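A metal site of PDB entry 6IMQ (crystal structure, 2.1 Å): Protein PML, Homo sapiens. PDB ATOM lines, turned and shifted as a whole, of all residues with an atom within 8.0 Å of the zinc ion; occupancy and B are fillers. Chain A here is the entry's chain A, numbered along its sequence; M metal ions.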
ATOM      1  N   VAL A  11       8.171  -7.824  24.974  1.00  0.00           N
ATOM      2  CA  VAL A  11       8.741  -9.115  24.612  1.00  0.00           C
ATOM      3  C   VAL A  11      10.205  -9.189  25.027  1.00  0.00           C
ATOM      4  O   VAL A  11      10.947  -8.204  24.982  1.00  0.00           O
ATOM      5  CB  VAL A  11       8.594  -9.406  23.106  1.00  0.00           C
ATOM      6  CG1 VAL A  11       7.119  -9.593  22.744  1.00  0.00           C
ATOM      7  CG2 VAL A  11       9.206  -8.296  22.284  1.00  0.00           C
ATOM      8  N   CYS A  12      10.612 -10.390  25.418  1.00  0.00           N
ATOM      9  CA  CYS A  12      11.962 -10.647  25.879  1.00  0.00           C
ATOM     10  C   CYS A  12      13.003 -10.223  24.850  1.00  0.00           C
ATOM     11  O   CYS A  12      12.920 -10.579  23.668  1.00  0.00           O
ATOM     12  CB  CYS A  12      12.114 -12.140  26.187  1.00  0.00           C
ATOM     13  SG  CYS A  12      13.746 -12.567  26.814  1.00  0.00           S
ATOM     14  N   THR A  13      13.990  -9.455  25.312  1.00  0.00           N
ATOM     15  CA  THR A  13      15.053  -8.996  24.427  1.00  0.00           C
ATOM     16  C   THR A  13      15.858 -10.156  23.865  1.00  0.00           C
ATOM     17  O   THR A  13      16.404 -10.053  22.757  1.00  0.00           O
ATOM     18  CB  THR A  13      15.978  -8.044  25.189  1.00  0.00           C
ATOM     19  OG1 THR A  13      15.189  -7.031  25.829  1.00  0.00           O
ATOM     20  CG2 THR A  13      16.957  -7.388  24.232  1.00  0.00           C
ATOM     21  N   ARG A  14      15.956 -11.270  24.592  1.00  0.00           N
ATOM     22  CA  ARG A  14      16.799 -12.375  24.158  1.00  0.00           C
ATOM     23  C   ARG A  14      16.073 -13.313  23.194  1.00  0.00           C
ATOM     24  O   ARG A  14      16.564 -13.573  22.090  1.00  0.00           O
ATOM     25  CB  ARG A  14      17.276 -13.169  25.379  1.00  0.00           C
ATOM     26  CG  ARG A  14      18.173 -14.369  25.056  1.00  0.00           C
ATOM     27  CD  ARG A  14      18.904 -14.922  26.286  1.00  0.00           C
ATOM     28  NE  ARG A  14      19.333 -16.298  26.018  1.00  0.00           N
ATOM     29  CZ  ARG A  14      18.878 -17.378  26.644  1.00  0.00           C
ATOM     30  NH1 ARG A  14      17.978 -17.276  27.616  1.00  0.00           N
ATOM     31  NH2 ARG A  14      19.338 -18.584  26.303  1.00  0.00           N
ATOM     32  N   CYS A  15      14.896 -13.779  23.574  1.00  0.00           N
ATOM     33  CA  CYS A  15      14.214 -14.848  22.865  1.00  0.00           C
ATOM     34  C   CYS A  15      12.896 -14.445  22.214  1.00  0.00           C
ATOM     35  O   CYS A  15      12.356 -15.241  21.447  1.00  0.00           O
ATOM     36  CB  CYS A  15      13.950 -16.032  23.816  1.00  0.00           C
ATOM     37  SG  CYS A  15      12.581 -15.762  24.967  1.00  0.00           S
ATOM     38  N   LYS A  16      12.390 -13.246  22.501  1.00  0.00           N
ATOM     39  CA  LYS A  16      11.204 -12.657  21.883  1.00  0.00           C
ATOM     40  C   LYS A  16       9.912 -13.294  22.408  1.00  0.00           C
ATOM     41  O   LYS A  16       8.846 -13.042  21.847  1.00  0.00           O
ATOM     42  CB  LYS A  16      11.250 -12.742  20.342  1.00  0.00           C
ATOM     43  CG  LYS A  16      12.580 -12.198  19.782  1.00  0.00           C
ATOM     44  CD  LYS A  16      12.772 -10.686  19.945  1.00  0.00           C
ATOM     45  CE  LYS A  16      12.000  -9.858  18.935  1.00  0.00           C
ATOM     46  NZ  LYS A  16      12.216 -10.287  17.530  1.00  0.00           N
ATOM     47  N   GLU A  17       9.977 -14.093  23.469  1.00  0.00           N
ATOM     48  CA  GLU A  17       8.779 -14.496  24.201  1.00  0.00           C
ATOM     49  C   GLU A  17       8.247 -13.298  24.991  1.00  0.00           C
ATOM     50  O   GLU A  17       8.909 -12.259  25.106  1.00  0.00           O
ATOM     51  CB  GLU A  17       9.119 -15.690  25.095  1.00  0.00           C
ATOM     52  CG  GLU A  17       8.021 -16.126  26.058  1.00  0.00           C
ATOM     53  CD  GLU A  17       6.816 -16.722  25.371  1.00  0.00           C
ATOM     54  OE1 GLU A  17       6.983 -17.555  24.445  1.00  0.00           O
ATOM     55  OE2 GLU A  17       5.687 -16.362  25.764  1.00  0.00           O
ATOM     56  N   SER A  18       7.020 -13.429  25.486  1.00  0.00           N
ATOM     57  CA  SER A  18       6.411 -12.356  26.266  1.00  0.00           C
ATOM     58  C   SER A  18       7.231 -12.065  27.523  1.00  0.00           C
ATOM     59  O   SER A  18       7.657 -12.976  28.236  1.00  0.00           O
ATOM     60  CB  SER A  18       4.977 -12.714  26.648  1.00  0.00           C
ATOM     61  OG  SER A  18       4.954 -13.558  27.780  1.00  0.00           O
ATOM     62  N   ALA A  19       7.423 -10.773  27.807  1.00  0.00           N
ATOM     63  CA  ALA A  19       8.351 -10.333  28.838  1.00  0.00           C
ATOM     64  C   ALA A  19       7.682 -10.209  30.199  1.00  0.00           C
ATOM     65  O   ALA A  19       6.487  -9.958  30.311  1.00  0.00           O
ATOM     66  CB  ALA A  19       8.962  -8.980  28.477  1.00  0.00           C
ATOM     67  N   ASP A  20       8.489 -10.390  31.252  1.00  0.00           N
ATOM     68  CA  ASP A  20       8.014 -10.343  32.629  1.00  0.00           C
ATOM     69  C   ASP A  20       8.831  -9.441  33.545  1.00  0.00           C
ATOM     70  O   ASP A  20       8.337  -9.098  34.626  1.00  0.00           O
ATOM     71  CB  ASP A  20       7.984 -11.757  33.223  1.00  0.00           C
ATOM     72  CG  ASP A  20       7.046 -12.687  32.464  1.00  0.00           C
ATOM     73  OD1 ASP A  20       5.857 -12.324  32.301  1.00  0.00           O
ATOM     74  OD2 ASP A  20       7.481 -13.774  32.032  1.00  0.00           O
ATOM     75  N   LEU A  29      14.389  -6.153  28.622  1.00  0.00           N
ATOM     76  CA  LEU A  29      13.202  -6.897  28.964  1.00  0.00           C
ATOM     77  C   LEU A  29      13.494  -8.392  28.886  1.00  0.00           C
ATOM     78  O   LEU A  29      14.064  -8.861  27.894  1.00  0.00           O
ATOM     79  CB  LEU A  29      12.071  -6.557  28.000  1.00  0.00           C
ATOM     80  CG  LEU A  29      11.585  -5.122  27.998  1.00  0.00           C
ATOM     81  CD1 LEU A  29      10.834  -4.862  26.712  1.00  0.00           C
ATOM     82  CD2 LEU A  29      10.740  -4.930  29.220  1.00  0.00           C
ATOM     83  N   LEU A  30      13.082  -9.142  29.909  1.00  0.00           N
ATOM     84  CA  LEU A  30      13.320 -10.578  29.966  1.00  0.00           C
ATOM     85  C   LEU A  30      12.048 -11.331  30.353  1.00  0.00           C
ATOM     86  O   LEU A  30      11.298 -10.899  31.228  1.00  0.00           O
ATOM     87  CB  LEU A  30      14.440 -10.872  30.970  1.00  0.00           C
ATOM     88  CG  LEU A  30      15.753 -10.188  30.607  1.00  0.00           C
ATOM     89  CD1 LEU A  30      16.754 -10.225  31.752  1.00  0.00           C
ATOM     90  CD2 LEU A  30      16.367 -10.835  29.345  1.00  0.00           C
ATOM     91  N   CYS A  31      11.837 -12.469  29.695  1.00  0.00           N
ATOM     92  CA  CYS A  31      10.830 -13.402  30.165  1.00  0.00           C
ATOM     93  C   CYS A  31      11.276 -14.035  31.483  1.00  0.00           C
ATOM     94  O   CYS A  31      12.441 -13.931  31.877  1.00  0.00           O
ATOM     95  CB  CYS A  31      10.580 -14.490  29.114  1.00  0.00           C
ATOM     96  SG  CYS A  31      11.987 -15.543  28.712  1.00  0.00           S
ATOM     97  N   ALA A  32      10.328 -14.698  32.152  1.00  0.00           N
ATOM     98  CA  ALA A  32      10.621 -15.368  33.418  1.00  0.00           C
ATOM     99  C   ALA A  32      11.784 -16.331  33.296  1.00  0.00           C
ATOM    100  O   ALA A  32      12.615 -16.420  34.211  1.00  0.00           O
ATOM    101  CB  ALA A  32       9.368 -16.097  33.907  1.00  0.00           C
ATOM    102  N   LYS A  33      11.838 -17.119  32.218  1.00  0.00           N
ATOM    103  CA  LYS A  33      12.885 -18.119  32.108  1.00  0.00           C
ATOM    104  C   LYS A  33      14.233 -17.493  31.811  1.00  0.00           C
ATOM    105  O   LYS A  33      15.250 -17.926  32.360  1.00  0.00           O
ATOM    106  CB  LYS A  33      12.493 -19.146  31.035  1.00  0.00           C
ATOM    107  CG  LYS A  33      11.503 -20.099  31.641  1.00  0.00           C
ATOM    108  CD  LYS A  33      11.563 -21.478  31.055  1.00  0.00           C
ATOM    109  CE  LYS A  33      11.040 -22.442  32.117  1.00  0.00           C
ATOM    110  NZ  LYS A  33       9.613 -22.233  32.479  1.00  0.00           N
ATOM    111  N   CYS A  34      14.276 -16.460  30.978  1.00  0.00           N
ATOM    112  CA  CYS A  34      15.527 -15.754  30.812  1.00  0.00           C
ATOM    113  C   CYS A  34      15.928 -15.027  32.087  1.00  0.00           C
ATOM    114  O   CYS A  34      17.115 -14.981  32.422  1.00  0.00           O
ATOM    115  CB  CYS A  34      15.440 -14.789  29.640  1.00  0.00           C
ATOM    116  SG  CYS A  34      15.482 -15.628  28.025  1.00  0.00           S
ATOM    117  N   PHE A  35      14.964 -14.516  32.860  1.00  0.00           N
ATOM    118  CA  PHE A  35      15.345 -13.777  34.053  1.00  0.00           C
ATOM    119  C   PHE A  35      15.914 -14.710  35.122  1.00  0.00           C
ATOM    120  O   PHE A  35      16.836 -14.325  35.845  1.00  0.00           O
ATOM    121  CB  PHE A  35      14.182 -12.976  34.640  1.00  0.00           C
ATOM    122  CG  PHE A  35      14.593 -12.062  35.752  1.00  0.00           C
ATOM    123  CD1 PHE A  35      15.412 -10.971  35.508  1.00  0.00           C
ATOM    124  CD2 PHE A  35      14.176 -12.292  37.055  1.00  0.00           C
ATOM    125  CE1 PHE A  35      15.813 -10.134  36.532  1.00  0.00           C
ATOM    126  CE2 PHE A  35      14.566 -11.448  38.084  1.00  0.00           C
ATOM    127  CZ  PHE A  35      15.395 -10.377  37.817  1.00  0.00           C
HETATM  128 ZN    ZN M   1      13.450 -14.811  27.073  1.00  0.00          ZN
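The side-chain sulfur of Cys 34 lies close to the guanidinium group of Arg 14 (3.0 Å). The side-chain sulfur (SG) of Cys 15 lies close to the backbone NH (N) of Glu 17, at 3.4 Å. The backbone NH (N) of Cys 12 lies within hydrogen-bond range of the backbone carbonyl oxygen (O) of Glu 17 (2.5 Å). The backbone NH of Arg 14 lies close to the side-chain sulfur of Cys 12 (3.4 Å).
Four residues have an atom within 4 Å of the zinc ion: Cys 12, Cys 15, Cys 31 and Cys 34. Along chain A the residues within 4 Å of the zinc ion span positions 12 to 34.
The zinc ion is bound by the side-chain sulfur (SG) of Cys 12, 2.3 Å away. The zinc ion is bound by SG of Cys 31 (2.3 Å). The side-chain sulfur (SG) of Cys 34 is bound to the zinc ion. SG of Cys 15 is bound to the zinc ion, at 2.5 Å.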
